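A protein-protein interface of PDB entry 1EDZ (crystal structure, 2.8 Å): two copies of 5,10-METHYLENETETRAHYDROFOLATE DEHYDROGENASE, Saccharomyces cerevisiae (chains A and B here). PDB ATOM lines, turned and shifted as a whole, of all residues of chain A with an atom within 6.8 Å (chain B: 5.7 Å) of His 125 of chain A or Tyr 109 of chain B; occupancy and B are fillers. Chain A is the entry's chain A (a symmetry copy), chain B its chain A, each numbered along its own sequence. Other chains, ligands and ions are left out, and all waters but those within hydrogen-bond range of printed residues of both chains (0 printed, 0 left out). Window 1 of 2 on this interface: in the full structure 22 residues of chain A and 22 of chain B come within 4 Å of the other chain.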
ATOM      1  N   GLN A 111      32.799  -6.771  32.911  1.00  0.00           N
ATOM      2  CA  GLN A 111      33.566  -7.070  31.707  1.00  0.00           C
ATOM      3  C   GLN A 111      33.463  -5.976  30.652  1.00  0.00           C
ATOM      4  O   GLN A 111      34.194  -5.989  29.666  1.00  0.00           O
ATOM      5  CB  GLN A 111      33.167  -8.425  31.112  1.00  0.00           C
ATOM      6  CG  GLN A 111      31.959  -8.409  30.206  1.00  0.00           C
ATOM      7  CD  GLN A 111      31.778  -9.718  29.456  1.00  0.00           C
ATOM      8  OE1 GLN A 111      31.570  -9.730  28.242  1.00  0.00           O
ATOM      9  NE2 GLN A 111      31.848 -10.826  30.179  1.00  0.00           N
ATOM     10  N   GLN A 112      32.550  -5.032  30.861  1.00  0.00           N
ATOM     11  CA  GLN A 112      32.370  -3.930  29.925  1.00  0.00           C
ATOM     12  C   GLN A 112      33.010  -2.650  30.460  1.00  0.00           C
ATOM     13  O   GLN A 112      33.053  -1.639  29.761  1.00  0.00           O
ATOM     14  CB  GLN A 112      30.876  -3.686  29.655  1.00  0.00           C
ATOM     15  CG  GLN A 112      30.071  -4.908  29.197  1.00  0.00           C
ATOM     16  CD  GLN A 112      30.560  -5.498  27.889  1.00  0.00           C
ATOM     17  OE1 GLN A 112      30.861  -4.779  26.937  1.00  0.00           O
ATOM     18  NE2 GLN A 112      30.622  -6.819  27.830  1.00  0.00           N
ATOM     19  N   ASP A 119      41.760  -4.458  27.259  1.00  0.00           N
ATOM     20  CA  ASP A 119      41.071  -5.704  27.576  1.00  0.00           C
ATOM     21  C   ASP A 119      41.787  -6.857  26.881  1.00  0.00           C
ATOM     22  O   ASP A 119      41.556  -7.127  25.702  1.00  0.00           O
ATOM     23  CB  ASP A 119      39.612  -5.622  27.129  1.00  0.00           C
ATOM     24  CG  ASP A 119      38.948  -6.976  27.033  1.00  0.00           C
ATOM     25  OD1 ASP A 119      39.245  -7.885  27.840  1.00  0.00           O
ATOM     26  OD2 ASP A 119      38.122  -7.135  26.120  1.00  0.00           O
ATOM     27  N   GLY A 122      39.415 -10.027  25.592  1.00  0.00           N
ATOM     28  CA  GLY A 122      38.346  -9.825  24.631  1.00  0.00           C
ATOM     29  C   GLY A 122      37.011  -9.918  25.343  1.00  0.00           C
ATOM     30  O   GLY A 122      36.047 -10.482  24.829  1.00  0.00           O
ATOM     31  N   LEU A 123      37.000  -9.430  26.574  1.00  0.00           N
ATOM     32  CA  LEU A 123      35.823  -9.418  27.422  1.00  0.00           C
ATOM     33  C   LEU A 123      34.785  -8.444  26.866  1.00  0.00           C
ATOM     34  O   LEU A 123      33.591  -8.744  26.837  1.00  0.00           O
ATOM     35  CB  LEU A 123      36.233  -8.978  28.830  1.00  0.00           C
ATOM     36  CG  LEU A 123      36.036  -9.921  30.016  1.00  0.00           C
ATOM     37  CD1 LEU A 123      36.586 -11.295  29.700  1.00  0.00           C
ATOM     38  CD2 LEU A 123      36.709  -9.327  31.244  1.00  0.00           C
ATOM     39  N   ASN A 124      35.253  -7.282  26.422  1.00  0.00           N
ATOM     40  CA  ASN A 124      34.394  -6.232  25.884  1.00  0.00           C
ATOM     41  C   ASN A 124      33.428  -6.732  24.817  1.00  0.00           C
ATOM     42  O   ASN A 124      33.781  -7.547  23.957  1.00  0.00           O
ATOM     43  CB  ASN A 124      35.245  -5.084  25.323  1.00  0.00           C
ATOM     44  CG  ASN A 124      34.414  -3.868  24.927  1.00  0.00           C
ATOM     45  OD1 ASN A 124      33.517  -3.949  24.083  1.00  0.00           O
ATOM     46  ND2 ASN A 124      34.725  -2.726  25.526  1.00  0.00           N
ATOM     47  N   HIS A 125      32.222  -6.176  24.848  1.00  0.00           N
ATOM     48  CA  HIS A 125      31.162  -6.531  23.918  1.00  0.00           C
ATOM     49  C   HIS A 125      31.553  -6.484  22.441  1.00  0.00           C
ATOM     50  O   HIS A 125      31.189  -7.381  21.682  1.00  0.00           O
ATOM     51  CB  HIS A 125      29.955  -5.623  24.154  1.00  0.00           C
ATOM     52  CG  HIS A 125      28.791  -5.908  23.259  1.00  0.00           C
ATOM     53  ND1 HIS A 125      28.475  -5.122  22.171  1.00  0.00           N
ATOM     54  CD2 HIS A 125      27.854  -6.887  23.300  1.00  0.00           C
ATOM     55  CE1 HIS A 125      27.396  -5.603  21.581  1.00  0.00           C
ATOM     56  NE2 HIS A 125      26.999  -6.671  22.247  1.00  0.00           N
ATOM     57  N   VAL A 126      32.287  -5.455  22.034  1.00  0.00           N
ATOM     58  CA  VAL A 126      32.678  -5.320  20.634  1.00  0.00           C
ATOM     59  C   VAL A 126      33.326  -6.570  20.051  1.00  0.00           C
ATOM     60  O   VAL A 126      32.980  -6.994  18.952  1.00  0.00           O
ATOM     61  CB  VAL A 126      33.600  -4.104  20.397  1.00  0.00           C
ATOM     62  CG1 VAL A 126      32.947  -2.845  20.932  1.00  0.00           C
ATOM     63  CG2 VAL A 126      34.956  -4.319  21.033  1.00  0.00           C
ATOM     64  N   TYR A 127      34.221  -7.191  20.809  1.00  0.00           N
ATOM     65  CA  TYR A 127      34.902  -8.391  20.333  1.00  0.00           C
ATOM     66  C   TYR A 127      33.906  -9.517  20.110  1.00  0.00           C
ATOM     67  O   TYR A 127      34.100 -10.383  19.254  1.00  0.00           O
ATOM     68  CB  TYR A 127      35.997  -8.792  21.322  1.00  0.00           C
ATOM     69  CG  TYR A 127      36.979  -7.669  21.540  1.00  0.00           C
ATOM     70  CD1 TYR A 127      37.092  -7.045  22.781  1.00  0.00           C
ATOM     71  CD2 TYR A 127      37.749  -7.181  20.482  1.00  0.00           C
ATOM     72  CE1 TYR A 127      37.943  -5.958  22.962  1.00  0.00           C
ATOM     73  CE2 TYR A 127      38.600  -6.099  20.651  1.00  0.00           C
ATOM     74  CZ  TYR A 127      38.692  -5.489  21.893  1.00  0.00           C
ATOM     75  OH  TYR A 127      39.517  -4.399  22.059  1.00  0.00           O
ATOM     76  N   TYR A 128      32.821  -9.480  20.868  1.00  0.00           N
ATOM     77  CA  TYR A 128      31.783 -10.478  20.731  1.00  0.00           C
ATOM     78  C   TYR A 128      30.971 -10.198  19.479  1.00  0.00           C
ATOM     79  O   TYR A 128      30.773 -11.092  18.653  1.00  0.00           O
ATOM     80  CB  TYR A 128      30.878 -10.484  21.959  1.00  0.00           C
ATOM     81  CG  TYR A 128      31.494 -11.191  23.134  1.00  0.00           C
ATOM     82  CD1 TYR A 128      31.912 -10.483  24.258  1.00  0.00           C
ATOM     83  CD2 TYR A 128      31.666 -12.574  23.120  1.00  0.00           C
ATOM     84  CE1 TYR A 128      32.488 -11.136  25.342  1.00  0.00           C
ATOM     85  CE2 TYR A 128      32.237 -13.237  24.192  1.00  0.00           C
ATOM     86  CZ  TYR A 128      32.648 -12.514  25.301  1.00  0.00           C
ATOM     87  OH  TYR A 128      33.230 -13.171  26.360  1.00  0.00           O
ATOM     88  N   GLN A 129      30.565  -8.942  19.306  1.00  0.00           N
ATOM     89  CA  GLN A 129      29.766  -8.559  18.147  1.00  0.00           C
ATOM     90  C   GLN A 129      30.541  -8.797  16.862  1.00  0.00           C
ATOM     91  O   GLN A 129      29.990  -9.315  15.882  1.00  0.00           O
ATOM     92  CB  GLN A 129      29.318  -7.096  18.226  1.00  0.00           C
ATOM     93  CG  GLN A 129      28.007  -6.856  17.495  1.00  0.00           C
ATOM     94  CD  GLN A 129      27.647  -5.391  17.339  1.00  0.00           C
ATOM     95  OE1 GLN A 129      27.495  -4.899  16.222  1.00  0.00           O
ATOM     96  NE2 GLN A 129      27.466  -4.698  18.453  1.00  0.00           N
ATOM     97  N   ASN A 130      31.824  -8.450  16.875  1.00  0.00           N
ATOM     98  CA  ASN A 130      32.683  -8.639  15.712  1.00  0.00           C
ATOM     99  C   ASN A 130      32.826 -10.120  15.394  1.00  0.00           C
ATOM    100  O   ASN A 130      33.019 -10.495  14.238  1.00  0.00           O
ATOM    101  CB  ASN A 130      34.056  -8.011  15.948  1.00  0.00           C
ATOM    102  CG  ASN A 130      33.980  -6.509  16.129  1.00  0.00           C
ATOM    103  OD1 ASN A 130      32.908  -5.919  16.028  1.00  0.00           O
ATOM    104  ND2 ASN A 130      35.111  -5.885  16.408  1.00  0.00           N
ATOM    105  N   LEU A 131      32.709 -10.961  16.419  1.00  0.00           N
ATOM    106  CA  LEU A 131      32.811 -12.403  16.245  1.00  0.00           C
ATOM    107  C   LEU A 131      31.575 -12.904  15.512  1.00  0.00           C
ATOM    108  O   LEU A 131      31.682 -13.603  14.502  1.00  0.00           O
ATOM    109  CB  LEU A 131      32.938 -13.100  17.606  1.00  0.00           C
ATOM    110  CG  LEU A 131      33.040 -14.632  17.611  1.00  0.00           C
ATOM    111  CD1 LEU A 131      34.033 -15.102  18.670  1.00  0.00           C
ATOM    112  CD2 LEU A 131      31.666 -15.262  17.823  1.00  0.00           C
ATOM    113  N   TYR A 132      30.410 -12.511  16.020  1.00  0.00           N
ATOM    114  CA  TYR A 132      29.117 -12.898  15.463  1.00  0.00           C
ATOM    115  C   TYR A 132      28.854 -12.390  14.054  1.00  0.00           C
ATOM    116  O   TYR A 132      28.171 -13.051  13.274  1.00  0.00           O
ATOM    117  CB  TYR A 132      27.984 -12.417  16.371  1.00  0.00           C
ATOM    118  CG  TYR A 132      27.776 -13.253  17.606  1.00  0.00           C
ATOM    119  CD1 TYR A 132      27.425 -12.664  18.817  1.00  0.00           C
ATOM    120  CD2 TYR A 132      27.888 -14.639  17.558  1.00  0.00           C
ATOM    121  CE1 TYR A 132      27.186 -13.434  19.943  1.00  0.00           C
ATOM    122  CE2 TYR A 132      27.653 -15.416  18.677  1.00  0.00           C
ATOM    123  CZ  TYR A 132      27.301 -14.810  19.863  1.00  0.00           C
ATOM    124  OH  TYR A 132      27.060 -15.592  20.964  1.00  0.00           O
ATOM    125  N   HIS A 133      29.332 -11.186  13.757  1.00  0.00           N
ATOM    126  CA  HIS A 133      29.140 -10.585  12.442  1.00  0.00           C
ATOM    127  C   HIS A 133      30.374 -10.806  11.576  1.00  0.00           C
ATOM    128  O   HIS A 133      30.600 -10.082  10.603  1.00  0.00           O
ATOM    129  CB  HIS A 133      28.868  -9.085  12.584  1.00  0.00           C
ATOM    130  CG  HIS A 133      27.706  -8.758  13.470  1.00  0.00           C
ATOM    131  ND1 HIS A 133      27.335  -7.463  13.761  1.00  0.00           N
ATOM    132  CD2 HIS A 133      26.833  -9.556  14.134  1.00  0.00           C
ATOM    133  CE1 HIS A 133      26.288  -7.473  14.566  1.00  0.00           C
ATOM    134  NE2 HIS A 133      25.966  -8.730  14.807  1.00  0.00           N
ATOM    135  N   GLU A 187      26.850 -16.504  27.594  1.00  0.00           N
ATOM    136  CA  GLU A 187      27.127 -15.339  26.771  1.00  0.00           C
ATOM    137  C   GLU A 187      28.632 -15.094  26.773  1.00  0.00           C
ATOM    138  O   GLU A 187      29.186 -14.517  25.839  1.00  0.00           O
ATOM    139  CB  GLU A 187      26.391 -14.122  27.336  1.00  0.00           C
ATOM    140  CG  GLU A 187      26.054 -13.064  26.300  1.00  0.00           C
ATOM    141  CD  GLU A 187      25.378 -13.651  25.069  1.00  0.00           C
ATOM    142  OE1 GLU A 187      26.012 -13.664  23.993  1.00  0.00           O
ATOM    143  OE2 GLU A 187      24.221 -14.112  25.168  1.00  0.00           O
ATOM    144  N   ARG A 191      27.767 -19.628  23.970  1.00  0.00           N
ATOM    145  CA  ARG A 191      27.185 -19.225  22.698  1.00  0.00           C
ATOM    146  C   ARG A 191      28.270 -18.798  21.699  1.00  0.00           C
ATOM    147  O   ARG A 191      28.281 -19.271  20.558  1.00  0.00           O
ATOM    148  CB  ARG A 191      26.166 -18.102  22.926  1.00  0.00           C
ATOM    149  CG  ARG A 191      25.122 -17.953  21.837  1.00  0.00           C
ATOM    150  CD  ARG A 191      24.000 -17.025  22.288  1.00  0.00           C
ATOM    151  NE  ARG A 191      24.429 -15.635  22.425  1.00  0.00           N
ATOM    152  CZ  ARG A 191      24.205 -14.689  21.515  1.00  0.00           C
ATOM    153  NH1 ARG A 191      23.555 -14.982  20.396  1.00  0.00           N
ATOM    154  NH2 ARG A 191      24.620 -13.447  21.723  1.00  0.00           N
ATOM    155  N   LYS A 225      26.098 -13.651   9.849  1.00  0.00           N
ATOM    156  CA  LYS A 225      26.040 -14.242  11.180  1.00  0.00           C
ATOM    157  C   LYS A 225      25.491 -15.660  11.121  1.00  0.00           C
ATOM    158  O   LYS A 225      24.532 -15.932  10.405  1.00  0.00           O
ATOM    159  CB  LYS A 225      25.140 -13.382  12.075  1.00  0.00           C
ATOM    160  CG  LYS A 225      24.727 -14.029  13.384  1.00  0.00           C
ATOM    161  CD  LYS A 225      23.591 -13.252  14.022  1.00  0.00           C
ATOM    162  CE  LYS A 225      23.047 -13.970  15.241  1.00  0.00           C
ATOM    163  NZ  LYS A 225      21.881 -13.260  15.834  1.00  0.00           N
ATOM    164  N   GLU B  80      18.314  -9.337  15.957  1.00  0.00           N
ATOM    165  CA  GLU B  80      19.625  -8.709  15.898  1.00  0.00           C
ATOM    166  C   GLU B  80      19.812  -8.057  14.536  1.00  0.00           C
ATOM    167  O   GLU B  80      19.936  -6.836  14.439  1.00  0.00           O
ATOM    168  CB  GLU B  80      20.711  -9.758  16.137  1.00  0.00           C
ATOM    169  CG  GLU B  80      22.108  -9.189  16.378  1.00  0.00           C
ATOM    170  CD  GLU B  80      23.103 -10.250  16.807  1.00  0.00           C
ATOM    171  OE1 GLU B  80      22.690 -11.266  17.406  1.00  0.00           O
ATOM    172  OE2 GLU B  80      24.305 -10.083  16.537  1.00  0.00           O
ATOM    173  N   ALA B 105      20.741 -13.695  29.219  1.00  0.00           N
ATOM    174  CA  ALA B 105      21.905 -12.875  28.925  1.00  0.00           C
ATOM    175  C   ALA B 105      21.804 -12.262  27.531  1.00  0.00           C
ATOM    176  O   ALA B 105      22.110 -11.084  27.347  1.00  0.00           O
ATOM    177  CB  ALA B 105      23.172 -13.696  29.057  1.00  0.00           C
ATOM    178  N   GLN B 106      21.322 -13.043  26.568  1.00  0.00           N
ATOM    179  CA  GLN B 106      21.176 -12.567  25.198  1.00  0.00           C
ATOM    180  C   GLN B 106      20.502 -11.204  25.121  1.00  0.00           C
ATOM    181  O   GLN B 106      20.866 -10.379  24.288  1.00  0.00           O
ATOM    182  CB  GLN B 106      20.410 -13.572  24.343  1.00  0.00           C
ATOM    183  CG  GLN B 106      21.207 -14.793  23.936  1.00  0.00           C
ATOM    184  CD  GLN B 106      20.839 -15.281  22.538  1.00  0.00           C
ATOM    185  OE1 GLN B 106      21.169 -14.642  21.536  1.00  0.00           O
ATOM    186  NE2 GLN B 106      20.156 -16.416  22.466  1.00  0.00           N
ATOM    187  N   ASP B 107      19.532 -10.961  25.998  1.00  0.00           N
ATOM    188  CA  ASP B 107      18.841  -9.676  26.016  1.00  0.00           C
ATOM    189  C   ASP B 107      19.817  -8.570  26.420  1.00  0.00           C
ATOM    190  O   ASP B 107      19.808  -7.474  25.846  1.00  0.00           O
ATOM    191  CB  ASP B 107      17.631  -9.718  26.960  1.00  0.00           C
ATOM    192  CG  ASP B 107      16.516 -10.617  26.447  1.00  0.00           C
ATOM    193  OD1 ASP B 107      15.349 -10.429  26.843  1.00  0.00           O
ATOM    194  OD2 ASP B 107      16.797 -11.528  25.648  1.00  0.00           O
ATOM    195  N   GLN B 108      20.700  -8.875  27.370  1.00  0.00           N
ATOM    196  CA  GLN B 108      21.695  -7.905  27.830  1.00  0.00           C
ATOM    197  C   GLN B 108      22.670  -7.651  26.685  1.00  0.00           C
ATOM    198  O   GLN B 108      23.247  -6.569  26.573  1.00  0.00           O
ATOM    199  CB  GLN B 108      22.456  -8.426  29.056  1.00  0.00           C
ATOM    200  CG  GLN B 108      21.607  -9.196  30.067  1.00  0.00           C
ATOM    201  CD  GLN B 108      20.292  -8.507  30.393  1.00  0.00           C
ATOM    202  OE1 GLN B 108      20.266  -7.343  30.801  1.00  0.00           O
ATOM    203  NE2 GLN B 108      19.192  -9.224  30.205  1.00  0.00           N
ATOM    204  N   TYR B 109      22.858  -8.669  25.850  1.00  0.00           N
ATOM    205  CA  TYR B 109      23.735  -8.577  24.688  1.00  0.00           C
ATOM    206  C   TYR B 109      23.048  -7.711  23.643  1.00  0.00           C
ATOM    207  O   TYR B 109      23.666  -6.812  23.061  1.00  0.00           O
ATOM    208  CB  TYR B 109      24.001  -9.972  24.109  1.00  0.00           C
ATOM    209  CG  TYR B 109      24.563  -9.980  22.699  1.00  0.00           C
ATOM    210  CD1 TYR B 109      25.900  -9.667  22.455  1.00  0.00           C
ATOM    211  CD2 TYR B 109      23.753 -10.292  21.608  1.00  0.00           C
ATOM    212  CE1 TYR B 109      26.415  -9.661  21.157  1.00  0.00           C
ATOM    213  CE2 TYR B 109      24.258 -10.289  20.308  1.00  0.00           C
ATOM    214  CZ  TYR B 109      25.588  -9.970  20.090  1.00  0.00           C
ATOM    215  OH  TYR B 109      26.093  -9.940  18.813  1.00  0.00           O
ATOM    216  N   LEU B 110      21.760  -7.974  23.431  1.00  0.00           N
ATOM    217  CA  LEU B 110      20.963  -7.245  22.456  1.00  0.00           C
ATOM    218  C   LEU B 110      20.912  -5.772  22.785  1.00  0.00           C
ATOM    219  O   LEU B 110      21.092  -4.937  21.902  1.00  0.00           O
ATOM    220  CB  LEU B 110      19.547  -7.815  22.375  1.00  0.00           C
ATOM    221  CG  LEU B 110      19.426  -9.194  21.719  1.00  0.00           C
ATOM    222  CD1 LEU B 110      18.010  -9.732  21.869  1.00  0.00           C
ATOM    223  CD2 LEU B 110      19.830  -9.110  20.254  1.00  0.00           C
ATOM    224  N   GLN B 111      20.758  -5.450  24.066  1.00  0.00           N
ATOM    225  CA  GLN B 111      20.689  -4.054  24.483  1.00  0.00           C
ATOM    226  C   GLN B 111      21.976  -3.289  24.204  1.00  0.00           C
ATOM    227  O   GLN B 111      22.015  -2.067  24.323  1.00  0.00           O
ATOM    228  CB  GLN B 111      20.304  -3.931  25.961  1.00  0.00           C
ATOM    229  CG  GLN B 111      21.444  -4.054  26.945  1.00  0.00           C
ATOM    230  CD  GLN B 111      21.037  -3.669  28.356  1.00  0.00           C
ATOM    231  OE1 GLN B 111      21.726  -2.900  29.027  1.00  0.00           O
ATOM    232  NE2 GLN B 111      19.918  -4.208  28.816  1.00  0.00           N
ATOM    233  N   GLN B 112      23.030  -4.010  23.836  1.00  0.00           N
ATOM    234  CA  GLN B 112      24.310  -3.385  23.532  1.00  0.00           C
ATOM    235  C   GLN B 112      24.535  -3.306  22.022  1.00  0.00           C
ATOM    236  O   GLN B 112      25.513  -2.714  21.571  1.00  0.00           O
ATOM    237  CB  GLN B 112      25.464  -4.163  24.186  1.00  0.00           C
ATOM    238  CG  GLN B 112      25.337  -4.406  25.694  1.00  0.00           C
ATOM    239  CD  GLN B 112      25.285  -3.129  26.510  1.00  0.00           C
ATOM    240  OE1 GLN B 112      26.041  -2.188  26.271  1.00  0.00           O
ATOM    241  NE2 GLN B 112      24.401  -3.098  27.494  1.00  0.00           N
ATOM    242  N   VAL B 113      23.665  -3.950  21.247  1.00  0.00           N
ATOM    243  CA  VAL B 113      23.789  -3.943  19.789  1.00  0.00           C
ATOM    244  C   VAL B 113      23.239  -2.642  19.188  1.00  0.00           C
ATOM    245  O   VAL B 113      23.787  -2.103  18.222  1.00  0.00           O
ATOM    246  CB  VAL B 113      23.055  -5.148  19.153  1.00  0.00           C
ATOM    247  CG1 VAL B 113      23.269  -5.164  17.650  1.00  0.00           C
ATOM    248  CG2 VAL B 113      23.544  -6.448  19.761  1.00  0.00           C
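Printed residues of chain B that touch a printed residue of chain A: Glu 80, Ala 105, Gln 106, Tyr 109, Gln 112 and Val 113. Hydrophobic or aromatic side chains of chain B that line the printed part of chain A: Ala 105 and Tyr 109. Of the 18 printed residues of chain A, 7 touch a printed residue of chain B. Hydrophobic or aromatic side chains of chain A within 4 Å of the printed part of chain B: His 125, Tyr 132 and His 133. Among the printed residues, 11 pairs touch across the chains. Among the printed residues, Asp or Glu carboxylates within 4 Å of a Lys or Arg side-chain nitrogen of the other chain: Lys 225 of chain A with Glu 80 of chain B (2.7 Å).
OE2 of Glu 80 of chain B sits at hydrogen-bond distance from NE2 of His 133 of chain A (2.8 Å). The side-chain carboxylate (OE1) of Glu 80 of chain B is in salt-bridge range of the side-chain amino group (NZ) of Lys 225 of chain A (2.7 Å). The side-chain carboxylate (OE2) of Glu 187 of chain A sits close to the backbone NH (N) of Gln 106 of chain B. OE1 of Gln 106 of chain B is in hydrogen-bond range of NH1 of Arg 191 of chain A, 2.7 Å away. A ring nitrogen (NE2) of His 125 of chain A lies close to the backbone carbonyl oxygen of Tyr 109 of chain B (3.4 Å).
Gln 112 of chain B touches His 125 of chain A (O to CE1, 3.4 Å). Gln 129 of chain A touches Tyr 109 of chain B. NE2 of Gln 129 of chain A touches CA of Val 113 of chain B (3.98 Å). Tyr 132 of chain A touches Tyr 109 of chain B. CB of Ala 105 of chain B touches CB of Glu 187 of chain A, 3.7 Å away. Arg 191 of chain A touches Tyr 109 of chain B.
Of chain B, only Tyr 109 and Gln 112 come within 4 Å of His 125 of chain A. Of the printed residues of chain B, Glu 187 of chain A touches Ala 105 (3.7 Å) and Gln 106 (3.3 Å). Of the printed residues of chain B, Tyr 132 of chain A touches Tyr 109 (3.0 Å). Of the printed residues of chain A, Val 113 of chain B touches Gln 129. The nearest residue of chain B that does not touch His 125 of chain A is Val 113 of chain B (4.1 Å).
The side-chain carboxylate (OE2) of Glu 80 of chain B lies within hydrogen-bond range of the side-chain hydroxyl (OH) of Tyr 109 of chain B (2.9 Å). The side-chain amide oxygen (OE1) of Gln 111 of chain B lies within hydrogen-bond range of the side-chain amide nitrogen (NE2) of Gln 112 of chain B (3.1 Å). The side-chain amide oxygen (OE1) of Gln 112 of chain A sits at hydrogen-bond distance from the backbone NH (N) of His 125 of chain A, 2.9 Å away. The guanidinium group of Arg 191 of chain A lies within hydrogen-bond range of the side-chain hydroxyl of Tyr 132 of chain A (3.0 Å). The side-chain carboxylate (OE1) of Glu 187 of chain A lies within salt-bridge range of the guanidinium group (NH2) of Arg 191 of chain A, 2.7 Å away.
Positions printed for both chains: 111 and 112. Of the 11 pairs that touch across the chains among the printed residues, none has its exchanged pair printed and touching as well.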
